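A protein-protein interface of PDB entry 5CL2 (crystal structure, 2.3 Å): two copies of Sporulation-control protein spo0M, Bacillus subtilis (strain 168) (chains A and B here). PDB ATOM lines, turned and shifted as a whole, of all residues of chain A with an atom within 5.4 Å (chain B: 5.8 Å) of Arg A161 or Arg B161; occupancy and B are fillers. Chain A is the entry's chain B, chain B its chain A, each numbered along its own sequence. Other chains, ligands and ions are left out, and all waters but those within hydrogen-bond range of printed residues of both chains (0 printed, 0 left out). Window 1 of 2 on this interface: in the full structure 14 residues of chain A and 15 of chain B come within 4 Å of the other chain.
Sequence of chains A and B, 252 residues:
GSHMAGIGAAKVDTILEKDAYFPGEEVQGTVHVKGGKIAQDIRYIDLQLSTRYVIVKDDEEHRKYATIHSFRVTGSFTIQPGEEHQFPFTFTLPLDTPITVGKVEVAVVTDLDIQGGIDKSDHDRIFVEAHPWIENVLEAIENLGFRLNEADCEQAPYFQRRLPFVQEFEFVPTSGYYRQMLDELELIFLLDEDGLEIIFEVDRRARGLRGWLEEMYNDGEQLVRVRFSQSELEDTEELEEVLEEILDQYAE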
ATOM      1  N   ALA A 156     -19.464  -0.760   1.048  1.00  0.00           N
ATOM      2  CA  ALA A 156     -19.267   0.685   0.905  1.00  0.00           C
ATOM      3  C   ALA A 156     -20.357   1.387   0.095  1.00  0.00           C
ATOM      4  O   ALA A 156     -20.055   2.001  -0.936  1.00  0.00           O
ATOM      5  CB  ALA A 156     -17.920   0.946   0.268  1.00  0.00           C
ATOM      6  N   PHE A 159     -20.014   5.390  -0.961  1.00  0.00           N
ATOM      7  CA  PHE A 159     -19.245   5.913  -2.098  1.00  0.00           C
ATOM      8  C   PHE A 159     -19.917   5.737  -3.439  1.00  0.00           C
ATOM      9  O   PHE A 159     -19.448   6.309  -4.423  1.00  0.00           O
ATOM     10  CB  PHE A 159     -17.871   5.260  -2.155  1.00  0.00           C
ATOM     11  CG  PHE A 159     -17.024   5.584  -0.979  1.00  0.00           C
ATOM     12  CD1 PHE A 159     -16.700   6.903  -0.696  1.00  0.00           C
ATOM     13  CD2 PHE A 159     -16.535   4.584  -0.153  1.00  0.00           C
ATOM     14  CE1 PHE A 159     -15.917   7.219   0.407  1.00  0.00           C
ATOM     15  CE2 PHE A 159     -15.737   4.898   0.943  1.00  0.00           C
ATOM     16  CZ  PHE A 159     -15.434   6.207   1.225  1.00  0.00           C
ATOM     17  N   GLN A 160     -21.003   4.954  -3.477  1.00  0.00           N
ATOM     18  CA  GLN A 160     -21.806   4.772  -4.701  1.00  0.00           C
ATOM     19  C   GLN A 160     -20.926   4.461  -5.922  1.00  0.00           C
ATOM     20  O   GLN A 160     -21.103   5.041  -6.996  1.00  0.00           O
ATOM     21  CB  GLN A 160     -22.658   6.017  -4.966  1.00  0.00           C
ATOM     22  CG  GLN A 160     -23.625   6.323  -3.828  1.00  0.00           C
ATOM     23  CD  GLN A 160     -24.561   7.477  -4.122  1.00  0.00           C
ATOM     24  OE1 GLN A 160     -24.891   7.762  -5.280  1.00  0.00           O
ATOM     25  NE2 GLN A 160     -24.988   8.161  -3.065  1.00  0.00           N
ATOM     26  N   ARG A 161     -20.003   3.520  -5.727  1.00  0.00           N
ATOM     27  CA  ARG A 161     -19.039   3.089  -6.729  1.00  0.00           C
ATOM     28  C   ARG A 161     -19.653   2.099  -7.716  1.00  0.00           C
ATOM     29  O   ARG A 161     -20.829   1.708  -7.573  1.00  0.00           O
ATOM     30  CB  ARG A 161     -17.862   2.430  -6.002  1.00  0.00           C
ATOM     31  CG  ARG A 161     -16.499   2.836  -6.495  1.00  0.00           C
ATOM     32  CD  ARG A 161     -16.202   4.267  -6.154  1.00  0.00           C
ATOM     33  NE  ARG A 161     -15.141   4.763  -7.032  1.00  0.00           N
ATOM     34  CZ  ARG A 161     -14.894   6.046  -7.271  1.00  0.00           C
ATOM     35  NH1 ARG A 161     -15.631   6.990  -6.702  1.00  0.00           N
ATOM     36  NH2 ARG A 161     -13.903   6.385  -8.085  1.00  0.00           N
ATOM     37  N   ARG A 162     -18.871   1.665  -8.702  1.00  0.00           N
ATOM     38  CA  ARG A 162     -19.344   0.618  -9.610  1.00  0.00           C
ATOM     39  C   ARG A 162     -19.610  -0.666  -8.824  1.00  0.00           C
ATOM     40  O   ARG A 162     -20.634  -1.324  -9.015  1.00  0.00           O
ATOM     41  CB  ARG A 162     -18.336   0.346 -10.725  1.00  0.00           C
ATOM     42  CG  ARG A 162     -18.883  -0.552 -11.848  1.00  0.00           C
ATOM     43  CD  ARG A 162     -17.776  -0.879 -12.861  1.00  0.00           C
ATOM     44  NE  ARG A 162     -16.770  -1.787 -12.321  1.00  0.00           N
ATOM     45  CZ  ARG A 162     -16.752  -3.101 -12.528  1.00  0.00           C
ATOM     46  NH1 ARG A 162     -17.677  -3.651 -13.292  1.00  0.00           N
ATOM     47  NH2 ARG A 162     -15.770  -3.858 -12.026  1.00  0.00           N
ATOM     48  N   LEU A 163     -18.660  -1.042  -7.964  1.00  0.00           N
ATOM     49  CA  LEU A 163     -18.855  -2.196  -7.090  1.00  0.00           C
ATOM     50  C   LEU A 163     -19.435  -1.761  -5.735  1.00  0.00           C
ATOM     51  O   LEU A 163     -19.268  -0.606  -5.334  1.00  0.00           O
ATOM     52  CB  LEU A 163     -17.531  -2.951  -6.934  1.00  0.00           C
ATOM     53  CG  LEU A 163     -16.949  -3.417  -8.274  1.00  0.00           C
ATOM     54  CD1 LEU A 163     -15.552  -4.051  -8.141  1.00  0.00           C
ATOM     55  CD2 LEU A 163     -17.918  -4.381  -8.950  1.00  0.00           C
ATOM     56  N   PRO A 164     -20.168  -2.672  -5.055  1.00  0.00           N
ATOM     57  CA  PRO A 164     -20.762  -2.443  -3.727  1.00  0.00           C
ATOM     58  C   PRO A 164     -19.726  -2.392  -2.590  1.00  0.00           C
ATOM     59  O   PRO A 164     -20.084  -2.081  -1.458  1.00  0.00           O
ATOM     60  CB  PRO A 164     -21.720  -3.638  -3.556  1.00  0.00           C
ATOM     61  CG  PRO A 164     -21.142  -4.694  -4.401  1.00  0.00           C
ATOM     62  CD  PRO A 164     -20.576  -3.976  -5.608  1.00  0.00           C
ATOM     63  N   PHE A 165     -18.488  -2.776  -2.863  1.00  0.00           N
ATOM     64  CA  PHE A 165     -17.454  -2.806  -1.834  1.00  0.00           C
ATOM     65  C   PHE A 165     -16.239  -1.964  -2.235  1.00  0.00           C
ATOM     66  O   PHE A 165     -16.053  -1.658  -3.420  1.00  0.00           O
ATOM     67  CB  PHE A 165     -16.999  -4.237  -1.596  1.00  0.00           C
ATOM     68  CG  PHE A 165     -16.291  -4.832  -2.781  1.00  0.00           C
ATOM     69  CD1 PHE A 165     -14.916  -4.698  -2.927  1.00  0.00           C
ATOM     70  CD2 PHE A 165     -17.008  -5.454  -3.789  1.00  0.00           C
ATOM     71  CE1 PHE A 165     -14.268  -5.212  -4.034  1.00  0.00           C
ATOM     72  CE2 PHE A 165     -16.368  -5.978  -4.897  1.00  0.00           C
ATOM     73  CZ  PHE A 165     -14.996  -5.855  -5.025  1.00  0.00           C
ATOM     74  N   VAL A 166     -15.392  -1.637  -1.258  1.00  0.00           N
ATOM     75  CA  VAL A 166     -14.058  -1.118  -1.555  1.00  0.00           C
ATOM     76  C   VAL A 166     -13.054  -1.942  -0.775  1.00  0.00           C
ATOM     77  O   VAL A 166     -13.395  -2.555   0.230  1.00  0.00           O
ATOM     78  CB  VAL A 166     -13.881   0.388  -1.206  1.00  0.00           C
ATOM     79  CG1 VAL A 166     -14.818   1.249  -2.043  1.00  0.00           C
ATOM     80  CG2 VAL A 166     -14.090   0.629   0.282  1.00  0.00           C
ATOM     81  N   LEU A 190      -8.767   4.149  -5.232  1.00  0.00           N
ATOM     82  CA  LEU A 190      -9.628   4.181  -6.395  1.00  0.00           C
ATOM     83  C   LEU A 190      -8.785   4.462  -7.620  1.00  0.00           C
ATOM     84  O   LEU A 190      -8.483   5.613  -7.920  1.00  0.00           O
ATOM     85  CB  LEU A 190     -10.701   5.259  -6.231  1.00  0.00           C
ATOM     86  CG  LEU A 190     -11.444   5.287  -4.892  1.00  0.00           C
ATOM     87  CD1 LEU A 190     -12.288   6.544  -4.793  1.00  0.00           C
ATOM     88  CD2 LEU A 190     -12.288   4.027  -4.721  1.00  0.00           C
ATOM     89  N   GLU A 197      -7.036   7.857  -6.828  1.00  0.00           N
ATOM     90  CA  GLU A 197      -7.619   8.646  -5.755  1.00  0.00           C
ATOM     91  C   GLU A 197      -7.445   7.864  -4.444  1.00  0.00           C
ATOM     92  O   GLU A 197      -7.634   6.647  -4.413  1.00  0.00           O
ATOM     93  CB  GLU A 197      -9.096   8.956  -6.041  1.00  0.00           C
ATOM     94  CG  GLU A 197      -9.728   9.929  -5.059  1.00  0.00           C
ATOM     95  CD  GLU A 197     -10.984  10.576  -5.601  1.00  0.00           C
ATOM     96  OE1 GLU A 197     -11.253  10.444  -6.813  1.00  0.00           O
ATOM     97  OE2 GLU A 197     -11.710  11.220  -4.818  1.00  0.00           O
ATOM     98  N   ARG A 225     -10.017  13.093   1.168  1.00  0.00           N
ATOM     99  CA  ARG A 225     -10.058  12.458  -0.140  1.00  0.00           C
ATOM    100  C   ARG A 225      -9.160  13.191  -1.111  1.00  0.00           C
ATOM    101  O   ARG A 225      -9.388  14.356  -1.412  1.00  0.00           O
ATOM    102  CB  ARG A 225     -11.487  12.425  -0.658  1.00  0.00           C
ATOM    103  CG  ARG A 225     -11.693  11.407  -1.727  1.00  0.00           C
ATOM    104  CD  ARG A 225     -13.147  11.099  -1.902  1.00  0.00           C
ATOM    105  NE  ARG A 225     -13.377  10.523  -3.217  1.00  0.00           N
ATOM    106  CZ  ARG A 225     -14.532   9.989  -3.598  1.00  0.00           C
ATOM    107  NH1 ARG A 225     -15.553   9.950  -2.749  1.00  0.00           N
ATOM    108  NH2 ARG A 225     -14.664   9.490  -4.822  1.00  0.00           N
ATOM    109  N   ALA B 156     -19.190   6.380 -21.974  1.00  0.00           N
ATOM    110  CA  ALA B 156     -17.867   6.596 -21.367  1.00  0.00           C
ATOM    111  C   ALA B 156     -17.234   5.379 -20.646  1.00  0.00           C
ATOM    112  O   ALA B 156     -16.885   5.459 -19.459  1.00  0.00           O
ATOM    113  CB  ALA B 156     -17.942   7.785 -20.406  1.00  0.00           C
ATOM    114  N   PRO B 157     -16.979   4.286 -21.385  1.00  0.00           N
ATOM    115  CA  PRO B 157     -16.311   3.132 -20.771  1.00  0.00           C
ATOM    116  C   PRO B 157     -14.939   3.466 -20.216  1.00  0.00           C
ATOM    117  O   PRO B 157     -14.521   2.819 -19.259  1.00  0.00           O
ATOM    118  CB  PRO B 157     -16.175   2.133 -21.934  1.00  0.00           C
ATOM    119  CG  PRO B 157     -16.264   2.961 -23.172  1.00  0.00           C
ATOM    120  CD  PRO B 157     -17.224   4.076 -22.823  1.00  0.00           C
ATOM    121  N   PHE B 159     -13.839   5.770 -18.271  1.00  0.00           N
ATOM    122  CA  PHE B 159     -13.824   6.158 -16.855  1.00  0.00           C
ATOM    123  C   PHE B 159     -14.298   5.051 -15.907  1.00  0.00           C
ATOM    124  O   PHE B 159     -14.156   5.162 -14.680  1.00  0.00           O
ATOM    125  CB  PHE B 159     -14.681   7.397 -16.653  1.00  0.00           C
ATOM    126  CG  PHE B 159     -14.156   8.609 -17.364  1.00  0.00           C
ATOM    127  CD1 PHE B 159     -12.924   9.140 -17.030  1.00  0.00           C
ATOM    128  CD2 PHE B 159     -14.877   9.197 -18.383  1.00  0.00           C
ATOM    129  CE1 PHE B 159     -12.429  10.247 -17.699  1.00  0.00           C
ATOM    130  CE2 PHE B 159     -14.399  10.311 -19.032  1.00  0.00           C
ATOM    131  CZ  PHE B 159     -13.163  10.835 -18.697  1.00  0.00           C
ATOM    132  N   GLN B 160     -14.844   3.978 -16.474  1.00  0.00           N
ATOM    133  CA  GLN B 160     -15.263   2.822 -15.673  1.00  0.00           C
ATOM    134  C   GLN B 160     -16.102   3.191 -14.439  1.00  0.00           C
ATOM    135  O   GLN B 160     -15.858   2.688 -13.342  1.00  0.00           O
ATOM    136  CB  GLN B 160     -14.032   2.007 -15.234  1.00  0.00           C
ATOM    137  CG  GLN B 160     -13.218   1.426 -16.427  1.00  0.00           C
ATOM    138  CD  GLN B 160     -12.105   0.466 -16.017  1.00  0.00           C
ATOM    139  OE1 GLN B 160     -12.163  -0.185 -14.958  1.00  0.00           O
ATOM    140  NE2 GLN B 160     -11.084   0.353 -16.878  1.00  0.00           N
ATOM    141  N   ARG B 161     -17.088   4.065 -14.626  1.00  0.00           N
ATOM    142  CA  ARG B 161     -17.960   4.482 -13.525  1.00  0.00           C
ATOM    143  C   ARG B 161     -19.095   3.462 -13.288  1.00  0.00           C
ATOM    144  O   ARG B 161     -19.232   2.463 -14.012  1.00  0.00           O
ATOM    145  CB  ARG B 161     -18.577   5.851 -13.815  1.00  0.00           C
ATOM    146  CG  ARG B 161     -17.626   6.845 -14.440  1.00  0.00           C
ATOM    147  CD  ARG B 161     -16.586   7.214 -13.442  1.00  0.00           C
ATOM    148  NE  ARG B 161     -17.181   7.937 -12.325  1.00  0.00           N
ATOM    149  CZ  ARG B 161     -16.542   8.167 -11.183  1.00  0.00           C
ATOM    150  NH1 ARG B 161     -15.315   7.705 -11.027  1.00  0.00           N
ATOM    151  NH2 ARG B 161     -17.130   8.837 -10.199  1.00  0.00           N
ATOM    152  N   ARG B 162     -19.929   3.755 -12.297  1.00  0.00           N
ATOM    153  CA  ARG B 162     -21.087   2.928 -12.004  1.00  0.00           C
ATOM    154  C   ARG B 162     -21.995   2.862 -13.233  1.00  0.00           C
ATOM    155  O   ARG B 162     -22.384   1.775 -13.673  1.00  0.00           O
ATOM    156  CB  ARG B 162     -21.834   3.489 -10.801  1.00  0.00           C
ATOM    157  CG  ARG B 162     -22.892   2.541 -10.269  1.00  0.00           C
ATOM    158  CD  ARG B 162     -23.722   3.151  -9.148  1.00  0.00           C
ATOM    159  NE  ARG B 162     -24.597   4.234  -9.600  1.00  0.00           N
ATOM    160  CZ  ARG B 162     -25.868   4.070  -9.963  1.00  0.00           C
ATOM    161  NH1 ARG B 162     -26.390   2.855  -9.982  1.00  0.00           N
ATOM    162  NH2 ARG B 162     -26.604   5.113 -10.344  1.00  0.00           N
ATOM    163  N   LEU B 163     -22.276   4.019 -13.827  1.00  0.00           N
ATOM    164  CA  LEU B 163     -23.058   4.087 -15.062  1.00  0.00           C
ATOM    165  C   LEU B 163     -22.132   4.047 -16.294  1.00  0.00           C
ATOM    166  O   LEU B 163     -20.983   4.429 -16.218  1.00  0.00           O
ATOM    167  CB  LEU B 163     -23.895   5.356 -15.060  1.00  0.00           C
ATOM    168  CG  LEU B 163     -24.799   5.431 -13.835  1.00  0.00           C
ATOM    169  CD1 LEU B 163     -25.531   6.776 -13.812  1.00  0.00           C
ATOM    170  CD2 LEU B 163     -25.803   4.250 -13.877  1.00  0.00           C
ATOM    171  N   PRO B 164     -22.641   3.555 -17.424  1.00  0.00           N
ATOM    172  CA  PRO B 164     -21.920   3.460 -18.698  1.00  0.00           C
ATOM    173  C   PRO B 164     -21.650   4.803 -19.375  1.00  0.00           C
ATOM    174  O   PRO B 164     -20.896   4.853 -20.358  1.00  0.00           O
ATOM    175  CB  PRO B 164     -22.847   2.599 -19.557  1.00  0.00           C
ATOM    176  CG  PRO B 164     -24.253   2.804 -18.925  1.00  0.00           C
ATOM    177  CD  PRO B 164     -23.965   2.902 -17.464  1.00  0.00           C
ATOM    178  N   PHE B 165     -22.279   5.865 -18.885  1.00  0.00           N
ATOM    179  CA  PHE B 165     -22.158   7.186 -19.494  1.00  0.00           C
ATOM    180  C   PHE B 165     -21.667   8.269 -18.536  1.00  0.00           C
ATOM    181  O   PHE B 165     -21.672   8.082 -17.332  1.00  0.00           O
ATOM    182  CB  PHE B 165     -23.512   7.616 -20.063  1.00  0.00           C
ATOM    183  CG  PHE B 165     -24.560   7.802 -19.006  1.00  0.00           C
ATOM    184  CD1 PHE B 165     -24.692   9.015 -18.341  1.00  0.00           C
ATOM    185  CD2 PHE B 165     -25.412   6.749 -18.672  1.00  0.00           C
ATOM    186  CE1 PHE B 165     -25.657   9.174 -17.351  1.00  0.00           C
ATOM    187  CE2 PHE B 165     -26.370   6.904 -17.696  1.00  0.00           C
ATOM    188  CZ  PHE B 165     -26.485   8.120 -17.031  1.00  0.00           C
ATOM    189  N   VAL B 166     -21.245   9.416 -19.063  1.00  0.00           N
ATOM    190  CA  VAL B 166     -21.080  10.580 -18.192  1.00  0.00           C
ATOM    191  C   VAL B 166     -21.828  11.761 -18.783  1.00  0.00           C
ATOM    192  O   VAL B 166     -22.072  11.796 -19.989  1.00  0.00           O
ATOM    193  CB  VAL B 166     -19.581  10.971 -17.994  1.00  0.00           C
ATOM    194  CG1 VAL B 166     -18.838   9.854 -17.323  1.00  0.00           C
ATOM    195  CG2 VAL B 166     -18.936  11.325 -19.318  1.00  0.00           C
ATOM    196  N   LEU B 190     -18.205  14.713 -11.592  1.00  0.00           N
ATOM    197  CA  LEU B 190     -18.455  13.500 -10.834  1.00  0.00           C
ATOM    198  C   LEU B 190     -18.735  13.893  -9.391  1.00  0.00           C
ATOM    199  O   LEU B 190     -17.824  14.233  -8.629  1.00  0.00           O
ATOM    200  CB  LEU B 190     -17.253  12.561 -10.922  1.00  0.00           C
ATOM    201  CG  LEU B 190     -16.717  12.350 -12.341  1.00  0.00           C
ATOM    202  CD1 LEU B 190     -15.394  11.594 -12.318  1.00  0.00           C
ATOM    203  CD2 LEU B 190     -17.750  11.593 -13.154  1.00  0.00           C
ATOM    204  N   ARG B 225      -7.660  16.309 -14.571  1.00  0.00           N
ATOM    205  CA  ARG B 225      -8.622  15.764 -13.635  1.00  0.00           C
ATOM    206  C   ARG B 225      -8.389  16.294 -12.228  1.00  0.00           C
ATOM    207  O   ARG B 225      -7.397  15.962 -11.602  1.00  0.00           O
ATOM    208  CB  ARG B 225      -8.552  14.234 -13.664  1.00  0.00           C
ATOM    209  CG  ARG B 225      -9.808  13.569 -13.162  1.00  0.00           C
ATOM    210  CD  ARG B 225      -9.894  12.116 -13.602  1.00  0.00           C
ATOM    211  NE  ARG B 225     -10.817  11.388 -12.735  1.00  0.00           N
ATOM    212  CZ  ARG B 225     -11.253  10.151 -12.962  1.00  0.00           C
ATOM    213  NH1 ARG B 225     -10.861   9.487 -14.043  1.00  0.00           N
ATOM    214  NH2 ARG B 225     -12.085   9.581 -12.104  1.00  0.00           N
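Gln A160 touches Arg B162, but with the chains exchanged Arg A162 does not touch Gln B160 (4.1 Å). Arg B161 touches its own counterpart, Arg A161. Arg A161 touches Arg B162, and with the chains exchanged Arg A162 touches Arg B161. Arg B162 touches its own counterpart, Arg A162. Of the 5 pairs that touch across the chains among the printed residues, 4 have their exchanged pair printed and touching as well.
Among the printed residues, merely in contact across the chains: Gln A160 with Arg B162 (3.9 Å), Arg A161 with Arg B161 (3.5 Å), Arg A161 with Arg B162 (3.5 Å), Arg A162 with Arg B161 (3.7 Å) and Arg A162 with Arg B162 (3.8 Å).
Of the 12 printed residues of chain A, 3 touch a printed residue of chain B. Printed residues of chain A that touch a printed residue of chain B: Gln A160, Arg A161 and Arg A162. Among the printed residues, no Asp or Glu carboxylate lies within 4 Å of a Lys or Arg side-chain nitrogen of the other chain.
Arg A161 touches just these residues of chain B: Arg B161 (3.5 Å) and Arg B162 (3.5 Å). Of chain A, only Arg A161 and Arg A162 come within 4 Å of Arg B161. Of the printed residues of chain B, Arg A162 touches Arg B161 (3.7 Å) and Arg B162 (3.8 Å). Of the printed residues of chain A, Arg B162 touches Gln A160, Arg A161 and Arg A162. Of the printed residues of chain B, Gln A160 touches Arg B162 (3.9 Å).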
